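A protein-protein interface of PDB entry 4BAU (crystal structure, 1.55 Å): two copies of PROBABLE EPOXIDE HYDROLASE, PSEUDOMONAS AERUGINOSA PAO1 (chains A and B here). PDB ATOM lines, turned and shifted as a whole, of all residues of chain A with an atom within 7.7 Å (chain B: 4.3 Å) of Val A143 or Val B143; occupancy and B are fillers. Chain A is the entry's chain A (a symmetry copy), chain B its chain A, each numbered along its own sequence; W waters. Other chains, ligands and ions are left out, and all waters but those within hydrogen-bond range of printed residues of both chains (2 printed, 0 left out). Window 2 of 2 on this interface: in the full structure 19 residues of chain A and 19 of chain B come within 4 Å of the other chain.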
ATOM      1  N   ILE A 136      34.715  20.599 -16.397  1.00  0.00           N
ATOM      2  CA  ILE A 136      34.491  19.482 -15.475  1.00  0.00           C
ATOM      3  C   ILE A 136      34.044  19.943 -14.099  1.00  0.00           C
ATOM      4  O   ILE A 136      33.226  19.277 -13.444  1.00  0.00           O
ATOM      5  CB  ILE A 136      35.675  18.499 -15.437  1.00  0.00           C
ATOM      6  CG1 ILE A 136      35.195  17.058 -15.103  1.00  0.00           C
ATOM      7  CG2 ILE A 136      36.766  18.943 -14.497  1.00  0.00           C
ATOM      8  CD1 ILE A 136      34.492  16.268 -16.262  1.00  0.00           C
ATOM      9  N   LEU A 137      34.593  21.078 -13.637  1.00  0.00           N
ATOM     10  CA  LEU A 137      34.130  21.615 -12.355  1.00  0.00           C
ATOM     11  C   LEU A 137      32.617  21.778 -12.299  1.00  0.00           C
ATOM     12  O   LEU A 137      31.966  21.406 -11.327  1.00  0.00           O
ATOM     13  CB  LEU A 137      34.881  22.911 -12.034  1.00  0.00           C
ATOM     14  CG  LEU A 137      34.912  23.393 -10.612  1.00  0.00           C
ATOM     15  CD1 LEU A 137      35.661  22.321  -9.757  1.00  0.00           C
ATOM     16  CD2 LEU A 137      35.590  24.754 -10.584  1.00  0.00           C
ATOM     17  N   ASP A 138      32.066  22.360 -13.348  1.00  0.00           N
ATOM     18  CA  ASP A 138      30.610  22.552 -13.492  1.00  0.00           C
ATOM     19  C   ASP A 138      29.879  21.206 -13.585  1.00  0.00           C
ATOM     20  O   ASP A 138      28.825  21.023 -12.927  1.00  0.00           O
ATOM     21  CB  ASP A 138      30.314  23.484 -14.642  1.00  0.00           C
ATOM     22  CG  ASP A 138      30.910  24.845 -14.430  1.00  0.00           C
ATOM     23  OD1 ASP A 138      30.333  25.622 -13.681  1.00  0.00           O
ATOM     24  OD2 ASP A 138      32.007  25.098 -14.944  1.00  0.00           O
ATOM     25  N   ASN A 139      30.407  20.249 -14.340  1.00  0.00           N
ATOM     26  CA  ASN A 139      29.797  18.890 -14.431  1.00  0.00           C
ATOM     27  C   ASN A 139      29.700  18.219 -13.061  1.00  0.00           C
ATOM     28  O   ASN A 139      28.613  17.696 -12.689  1.00  0.00           O
ATOM     29  CB  ASN A 139      30.554  17.953 -15.377  1.00  0.00           C
ATOM     30  CG  ASN A 139      30.575  18.416 -16.830  1.00  0.00           C
ATOM     31  OD1 ASN A 139      31.665  18.453 -17.426  1.00  0.00           O
ATOM     32  ND2 ASN A 139      29.418  18.633 -17.428  1.00  0.00           N
ATOM     33  N   TRP A 140      30.793  18.268 -12.274  1.00  0.00           N
ATOM     34  CA  TRP A 140      30.748  17.583 -11.008  1.00  0.00           C
ATOM     35  C   TRP A 140      29.726  18.202 -10.072  1.00  0.00           C
ATOM     36  O   TRP A 140      29.068  17.467  -9.308  1.00  0.00           O
ATOM     37  CB  TRP A 140      32.108  17.509 -10.337  1.00  0.00           C
ATOM     38  CG  TRP A 140      33.138  16.647 -11.032  1.00  0.00           C
ATOM     39  CD1 TRP A 140      34.486  16.930 -11.218  1.00  0.00           C
ATOM     40  CD2 TRP A 140      32.954  15.312 -11.642  1.00  0.00           C
ATOM     41  NE1 TRP A 140      35.124  15.917 -11.865  1.00  0.00           N
ATOM     42  CE2 TRP A 140      34.246  14.923 -12.185  1.00  0.00           C
ATOM     43  CE3 TRP A 140      31.893  14.433 -11.773  1.00  0.00           C
ATOM     44  CZ2 TRP A 140      34.435  13.705 -12.829  1.00  0.00           C
ATOM     45  CZ3 TRP A 140      32.082  13.215 -12.443  1.00  0.00           C
ATOM     46  CH2 TRP A 140      33.330  12.844 -12.942  1.00  0.00           C
ATOM     47  N   ALA A 141      29.574  19.525 -10.119  1.00  0.00           N
ATOM     48  CA  ALA A 141      28.617  20.185  -9.250  1.00  0.00           C
ATOM     49  C   ALA A 141      27.170  19.804  -9.561  1.00  0.00           C
ATOM     50  O   ALA A 141      26.285  19.929  -8.710  1.00  0.00           O
ATOM     51  CB  ALA A 141      28.824  21.716  -9.351  1.00  0.00           C
ATOM     52  N   ALA A 142      26.947  19.326 -10.771  1.00  0.00           N
ATOM     53  CA  ALA A 142      25.606  18.988 -11.294  1.00  0.00           C
ATOM     54  C   ALA A 142      25.214  17.534 -11.028  1.00  0.00           C
ATOM     55  O   ALA A 142      24.138  17.088 -11.418  1.00  0.00           O
ATOM     56  CB  ALA A 142      25.553  19.256 -12.801  1.00  0.00           C
ATOM     57  N   VAL A 143      26.109  16.761 -10.447  1.00  0.00           N
ATOM     58  CA  VAL A 143      25.811  15.309 -10.268  1.00  0.00           C
ATOM     59  C   VAL A 143      24.599  15.098  -9.382  1.00  0.00           C
ATOM     60  O   VAL A 143      24.574  15.566  -8.268  1.00  0.00           O
ATOM     61  CB  VAL A 143      27.037  14.521  -9.743  1.00  0.00           C
ATOM     62  CG1 VAL A 143      26.678  13.028  -9.481  1.00  0.00           C
ATOM     63  CG2 VAL A 143      28.137  14.554 -10.772  1.00  0.00           C
ATOM     64  N   ASN A 144      23.662  14.270  -9.851  1.00  0.00           N
ATOM     65  CA  ASN A 144      22.521  13.818  -9.114  1.00  0.00           C
ATOM     66  C   ASN A 144      22.194  12.426  -9.704  1.00  0.00           C
ATOM     67  O   ASN A 144      22.918  11.913 -10.555  1.00  0.00           O
ATOM     68  CB  ASN A 144      21.348  14.786  -9.226  1.00  0.00           C
ATOM     69  CG  ASN A 144      20.925  15.080 -10.656  1.00  0.00           C
ATOM     70  OD1 ASN A 144      21.200  14.328 -11.579  1.00  0.00           O
ATOM     71  ND2 ASN A 144      20.142  16.178 -10.810  1.00  0.00           N
ATOM     72  N   LYS A 145      21.113  11.812  -9.220  1.00  0.00           N
ATOM     73  CA  LYS A 145      20.702  10.467  -9.641  1.00  0.00           C
ATOM     74  C   LYS A 145      20.625  10.349 -11.162  1.00  0.00           C
ATOM     75  O   LYS A 145      21.260   9.501 -11.729  1.00  0.00           O
ATOM     76  CB  LYS A 145      19.361  10.121  -9.010  1.00  0.00           C
ATOM     77  CG  LYS A 145      18.865   8.736  -9.379  1.00  0.00           C
ATOM     78  CD  LYS A 145      17.366   8.653  -9.127  1.00  0.00           C
ATOM     79  CE  LYS A 145      16.759   7.312  -9.380  1.00  0.00           C
ATOM     80  NZ  LYS A 145      15.263   7.356  -9.294  1.00  0.00           N
ATOM     81  N   VAL A 146      19.911  11.274 -11.814  1.00  0.00           N
ATOM     82  CA  VAL A 146      19.746  11.221 -13.272  1.00  0.00           C
ATOM     83  C   VAL A 146      21.049  11.389 -14.025  1.00  0.00           C
ATOM     84  O   VAL A 146      21.287  10.674 -14.980  1.00  0.00           O
ATOM     85  CB  VAL A 146      18.622  12.180 -13.707  1.00  0.00           C
ATOM     86  CG1 VAL A 146      18.667  12.367 -15.213  1.00  0.00           C
ATOM     87  CG2 VAL A 146      17.263  11.704 -13.195  1.00  0.00           C
ATOM     88  N   PHE A 147      21.950  12.257 -13.541  1.00  0.00           N
ATOM     89  CA  PHE A 147      23.210  12.476 -14.214  1.00  0.00           C
ATOM     90  C   PHE A 147      23.991  11.173 -14.170  1.00  0.00           C
ATOM     91  O   PHE A 147      24.576  10.773 -15.168  1.00  0.00           O
ATOM     92  CB  PHE A 147      23.998  13.589 -13.473  1.00  0.00           C
ATOM     93  CG  PHE A 147      25.346  13.930 -14.058  1.00  0.00           C
ATOM     94  CD1 PHE A 147      26.408  13.077 -13.893  1.00  0.00           C
ATOM     95  CD2 PHE A 147      25.597  15.191 -14.632  1.00  0.00           C
ATOM     96  CE1 PHE A 147      27.667  13.389 -14.429  1.00  0.00           C
ATOM     97  CE2 PHE A 147      26.865  15.498 -15.109  1.00  0.00           C
ATOM     98  CZ  PHE A 147      27.891  14.581 -15.022  1.00  0.00           C
ATOM     99  N   ALA A 148      24.027  10.558 -12.982  1.00  0.00           N
ATOM    100  CA  ALA A 148      24.919   9.405 -12.753  1.00  0.00           C
ATOM    101  C   ALA A 148      24.406   8.181 -13.529  1.00  0.00           C
ATOM    102  O   ALA A 148      25.178   7.350 -13.965  1.00  0.00           O
ATOM    103  CB  ALA A 148      25.089   9.097 -11.249  1.00  0.00           C
ATOM    104  N   LEU A 149      23.098   8.087 -13.702  1.00  0.00           N
ATOM    105  CA  LEU A 149      22.520   7.022 -14.573  1.00  0.00           C
ATOM    106  C   LEU A 149      22.852   7.255 -16.057  1.00  0.00           C
ATOM    107  O   LEU A 149      23.200   6.313 -16.782  1.00  0.00           O
ATOM    108  CB  LEU A 149      21.021   6.889 -14.324  1.00  0.00           C
ATOM    109  CG  LEU A 149      20.618   6.274 -12.985  1.00  0.00           C
ATOM    110  CD1 LEU A 149      19.114   6.540 -12.691  1.00  0.00           C
ATOM    111  CD2 LEU A 149      20.950   4.770 -12.964  1.00  0.00           C
ATOM    112  N   TRP A 154      31.217   7.671 -16.626  1.00  0.00           N
ATOM    113  CA  TRP A 154      32.088   8.623 -15.958  1.00  0.00           C
ATOM    114  C   TRP A 154      32.543   8.112 -14.622  1.00  0.00           C
ATOM    115  O   TRP A 154      33.626   8.454 -14.147  1.00  0.00           O
ATOM    116  CB  TRP A 154      31.386   9.958 -15.760  1.00  0.00           C
ATOM    117  CG  TRP A 154      31.193  10.761 -17.006  1.00  0.00           C
ATOM    118  CD1 TRP A 154      30.994  10.293 -18.304  1.00  0.00           C
ATOM    119  CD2 TRP A 154      31.210  12.204 -17.094  1.00  0.00           C
ATOM    120  NE1 TRP A 154      30.927  11.342 -19.183  1.00  0.00           N
ATOM    121  CE2 TRP A 154      31.077  12.532 -18.503  1.00  0.00           C
ATOM    122  CE3 TRP A 154      31.426  13.225 -16.187  1.00  0.00           C
ATOM    123  CZ2 TRP A 154      31.040  13.852 -18.943  1.00  0.00           C
ATOM    124  CZ3 TRP A 154      31.383  14.549 -16.646  1.00  0.00           C
ATOM    125  CH2 TRP A 154      31.224  14.849 -17.968  1.00  0.00           C
ATOM    126  N   PHE A 155      31.672   7.328 -13.956  1.00  0.00           N
ATOM    127  CA  PHE A 155      31.961   6.722 -12.675  1.00  0.00           C
ATOM    128  C   PHE A 155      32.600   5.360 -12.779  1.00  0.00           C
ATOM    129  O   PHE A 155      33.536   5.071 -12.048  1.00  0.00           O
ATOM    130  CB  PHE A 155      30.638   6.749 -11.878  1.00  0.00           C
ATOM    131  CG  PHE A 155      30.103   8.151 -11.778  1.00  0.00           C
ATOM    132  CD1 PHE A 155      30.678   9.056 -10.904  1.00  0.00           C
ATOM    133  CD2 PHE A 155      29.091   8.562 -12.601  1.00  0.00           C
ATOM    134  CE1 PHE A 155      30.238  10.388 -10.876  1.00  0.00           C
ATOM    135  CE2 PHE A 155      28.648   9.843 -12.620  1.00  0.00           C
ATOM    136  CZ  PHE A 155      29.181  10.772 -11.707  1.00  0.00           C
ATOM    137  N   GLN A 253      22.955  25.708 -15.150  1.00  0.00           N
ATOM    138  CA  GLN A 253      23.563  24.666 -15.977  1.00  0.00           C
ATOM    139  C   GLN A 253      23.511  25.009 -17.508  1.00  0.00           C
ATOM    140  O   GLN A 253      24.016  24.245 -18.327  1.00  0.00           O
ATOM    141  CB  GLN A 253      22.969  23.235 -15.616  1.00  0.00           C
ATOM    142  CG  GLN A 253      23.305  22.729 -14.160  1.00  0.00           C
ATOM    143  CD  GLN A 253      22.582  21.455 -13.574  1.00  0.00           C
ATOM    144  OE1 GLN A 253      22.203  20.476 -14.285  1.00  0.00           O
ATOM    145  NE2 GLN A 253      22.459  21.443 -12.212  1.00  0.00           N
ATOM    146  N   ASN B 139      18.599   7.618  -0.190  1.00  0.00           N
ATOM    147  CA  ASN B 139      19.863   7.407  -0.955  1.00  0.00           C
ATOM    148  C   ASN B 139      19.894   8.236  -2.239  1.00  0.00           C
ATOM    149  O   ASN B 139      20.906   8.939  -2.512  1.00  0.00           O
ATOM    150  CB  ASN B 139      20.107   5.940  -1.319  1.00  0.00           C
ATOM    151  CG  ASN B 139      20.277   5.018  -0.117  1.00  0.00           C
ATOM    152  OD1 ASN B 139      19.608   3.972  -0.070  1.00  0.00           O
ATOM    153  ND2 ASN B 139      21.223   5.308   0.758  1.00  0.00           N
ATOM    154  N   TRP B 140      18.788   8.218  -3.010  1.00  0.00           N
ATOM    155  CA  TRP B 140      18.820   8.935  -4.257  1.00  0.00           C
ATOM    156  C   TRP B 140      18.961  10.431  -4.041  1.00  0.00           C
ATOM    157  O   TRP B 140      19.644  11.105  -4.838  1.00  0.00           O
ATOM    158  CB  TRP B 140      17.616   8.635  -5.133  1.00  0.00           C
ATOM    159  CG  TRP B 140      17.531   7.226  -5.675  1.00  0.00           C
ATOM    160  CD1 TRP B 140      16.399   6.427  -5.771  1.00  0.00           C
ATOM    161  CD2 TRP B 140      18.616   6.398  -6.244  1.00  0.00           C
ATOM    162  NE1 TRP B 140      16.685   5.221  -6.333  1.00  0.00           N
ATOM    163  CE2 TRP B 140      18.017   5.123  -6.608  1.00  0.00           C
ATOM    164  CE3 TRP B 140      19.965   6.585  -6.489  1.00  0.00           C
ATOM    165  CZ2 TRP B 140      18.762   4.100  -7.185  1.00  0.00           C
ATOM    166  CZ3 TRP B 140      20.718   5.542  -7.052  1.00  0.00           C
ATOM    167  CH2 TRP B 140      20.129   4.333  -7.415  1.00  0.00           C
ATOM    168  N   ALA B 141      18.342  10.957  -2.986  1.00  0.00           N
ATOM    169  CA  ALA B 141      18.431  12.382  -2.719  1.00  0.00           C
ATOM    170  C   ALA B 141      19.848  12.834  -2.368  1.00  0.00           C
ATOM    171  O   ALA B 141      20.191  14.011  -2.510  1.00  0.00           O
ATOM    172  CB  ALA B 141      17.436  12.741  -1.588  1.00  0.00           C
ATOM    173  N   ALA B 142      20.663  11.891  -1.933  1.00  0.00           N
ATOM    174  CA  ALA B 142      22.040  12.142  -1.458  1.00  0.00           C
ATOM    175  C   ALA B 142      23.081  12.038  -2.573  1.00  0.00           C
ATOM    176  O   ALA B 142      24.276  12.198  -2.339  1.00  0.00           O
ATOM    177  CB  ALA B 142      22.395  11.152  -0.345  1.00  0.00           C
ATOM    178  N   VAL B 143      22.656  11.683  -3.769  1.00  0.00           N
ATOM    179  CA  VAL B 143      23.651  11.462  -4.859  1.00  0.00           C
ATOM    180  C   VAL B 143      24.424  12.729  -5.170  1.00  0.00           C
ATOM    181  O   VAL B 143      23.833  13.738  -5.479  1.00  0.00           O
ATOM    182  CB  VAL B 143      22.999  10.872  -6.135  1.00  0.00           C
ATOM    183  CG1 VAL B 143      24.038  10.733  -7.287  1.00  0.00           C
ATOM    184  CG2 VAL B 143      22.458   9.499  -5.838  1.00  0.00           C
ATOM    185  N   ASN B 144      25.752  12.614  -5.215  1.00  0.00           N
ATOM    186  CA  ASN B 144      26.653  13.644  -5.637  1.00  0.00           C
ATOM    187  C   ASN B 144      27.874  12.891  -6.216  1.00  0.00           C
ATOM    188  O   ASN B 144      27.874  11.666  -6.312  1.00  0.00           O
ATOM    189  CB  ASN B 144      27.035  14.574  -4.490  1.00  0.00           C
ATOM    190  CG  ASN B 144      27.634  13.860  -3.290  1.00  0.00           C
ATOM    191  OD1 ASN B 144      28.135  12.750  -3.382  1.00  0.00           O
ATOM    192  ND2 ASN B 144      27.658  14.585  -2.142  1.00  0.00           N
ATOM    193  N   LYS B 145      28.898  13.641  -6.625  1.00  0.00           N
ATOM    194  CA  LYS B 145      30.104  13.078  -7.245  1.00  0.00           C
ATOM    195  C   LYS B 145      30.699  11.952  -6.402  1.00  0.00           C
ATOM    196  O   LYS B 145      30.870  10.866  -6.889  1.00  0.00           O
ATOM    197  CB  LYS B 145      31.130  14.180  -7.463  1.00  0.00           C
ATOM    198  CG  LYS B 145      32.407  13.690  -8.117  1.00  0.00           C
ATOM    199  CD  LYS B 145      33.522  14.696  -7.866  1.00  0.00           C
ATOM    200  CE  LYS B 145      34.823  14.369  -8.522  1.00  0.00           C
ATOM    201  NZ  LYS B 145      35.915  15.296  -8.078  1.00  0.00           N
ATOM    202  N   PHE B 147      29.341  10.124  -3.979  1.00  0.00           N
ATOM    203  CA  PHE B 147      28.462   8.991  -3.804  1.00  0.00           C
ATOM    204  C   PHE B 147      28.590   8.112  -5.038  1.00  0.00           C
ATOM    205  O   PHE B 147      28.678   6.896  -4.920  1.00  0.00           O
ATOM    206  CB  PHE B 147      27.000   9.494  -3.665  1.00  0.00           C
ATOM    207  CG  PHE B 147      25.958   8.420  -3.479  1.00  0.00           C
ATOM    208  CD1 PHE B 147      25.579   7.633  -4.537  1.00  0.00           C
ATOM    209  CD2 PHE B 147      25.229   8.306  -2.280  1.00  0.00           C
ATOM    210  CE1 PHE B 147      24.606   6.635  -4.376  1.00  0.00           C
ATOM    211  CE2 PHE B 147      24.234   7.344  -2.160  1.00  0.00           C
ATOM    212  CZ  PHE B 147      23.942   6.498  -3.208  1.00  0.00           C
ATOM    213  N   PHE B 155      24.834   2.534 -10.387  1.00  0.00           N
ATOM    214  CA  PHE B 155      24.561   3.102 -11.689  1.00  0.00           C
ATOM    215  C   PHE B 155      24.876   2.172 -12.834  1.00  0.00           C
ATOM    216  O   PHE B 155      24.099   2.080 -13.772  1.00  0.00           O
ATOM    217  CB  PHE B 155      25.310   4.452 -11.736  1.00  0.00           C
ATOM    218  CG  PHE B 155      24.894   5.334 -10.590  1.00  0.00           C
ATOM    219  CD1 PHE B 155      23.672   5.982 -10.619  1.00  0.00           C
ATOM    220  CD2 PHE B 155      25.688   5.445  -9.483  1.00  0.00           C
ATOM    221  CE1 PHE B 155      23.245   6.731  -9.511  1.00  0.00           C
ATOM    222  CE2 PHE B 155      25.306   6.143  -8.385  1.00  0.00           C
ATOM    223  CZ  PHE B 155      24.091   6.852  -8.405  1.00  0.00           C
HETATM  224  O   HOH W   1      28.629  16.601  -6.772  1.00  0.00           O
HETATM  225  O   HOH W   2      19.687  12.921  -6.856  1.00  0.00           O
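Trp A140 touches Lys B145, and with the chains exchanged Lys A145 touches Trp B140.
Val A143 touches its own counterpart, Val B143.
Val A143 touches Asn B144, and with the chains exchanged Asn A144 touches Val B143.
Val A143 touches Lys B145, and with the chains exchanged Lys A145 touches Val B143.
Positions printed for both chains: 139, 140, 141, 142, 143, 144, 145, 147 and 155.
Of the 9 pairs that touch across the chains among the printed residues, 7 have their exchanged pair printed and touching as well.
Of the printed residues of chain B, Trp A140 touches Lys B145 (3.7 Å).
Val A143 touches just these residues of chain B: Val B143 (3.4 Å), Asn B144 (3.5 Å) and Lys B145 (3.7 Å).
Printed residues of chain B within 4 Å of Asn A144: Val B143.
No residue of chain A comes within 4 Å of Ala B142.
Printed residues of chain A within 4 Å of Phe B155: Ala A148 (3.5 Å) and Leu A149 (3.8 Å).
The nearest residue of chain A that does not touch Val B143 is Ala A148 (4.4 Å).
The nearest printed residue of chain A that does not touch Trp B140 is Leu A149 (5.6 Å).
The backbone NH (N) of Phe B147 is in hydrogen-bond range of the side-chain amide oxygen (OD1) of Asn B144 (3.0 Å).
OD1 of Asn A144 sits close to N of Val A146, at 3.3 Å.
The side-chain amide oxygen (OD1) of Asn A144 is in hydrogen-bond range of the backbone NH (N) of Phe A147 (2.9 Å).
Of the 17 printed residues of chain A, 6 touch a printed residue of chain B.
Hydrophobic or aromatic side chains of chain A within 4 Å of the printed part of chain B: Trp A140, Val A143, Ala A148 and Leu A149.
Of the 9 printed residues of chain B, 5 touch a printed residue of chain A.
Among the printed residues, 9 pairs touch across the chains.
Among the printed residues, no Asp or Glu carboxylate lies within 4 Å of a Lys or Arg side-chain nitrogen of the other chain.
Among the printed residues, pairs that only touch across the chains: Trp A140 with Lys B145, Val A143 with Asn B144, Val A143 with Lys B145, Asn A144 with Val B143, Lys A145 with Trp B140, Lys A145 with Val B143, Ala A148 with Phe B155 and Leu A149 with Phe B155.
Water W2 bridges the backbone carbonyl oxygen of Trp B140 (2.7 Å) and the backbone NH of Lys A145 (3.0 Å).
Water W1 lies within hydrogen-bond range of O of Trp A140 (2.7 Å) and N of Lys B145 (3.0 Å).
O of Val B143 sits close to O of Val A143.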
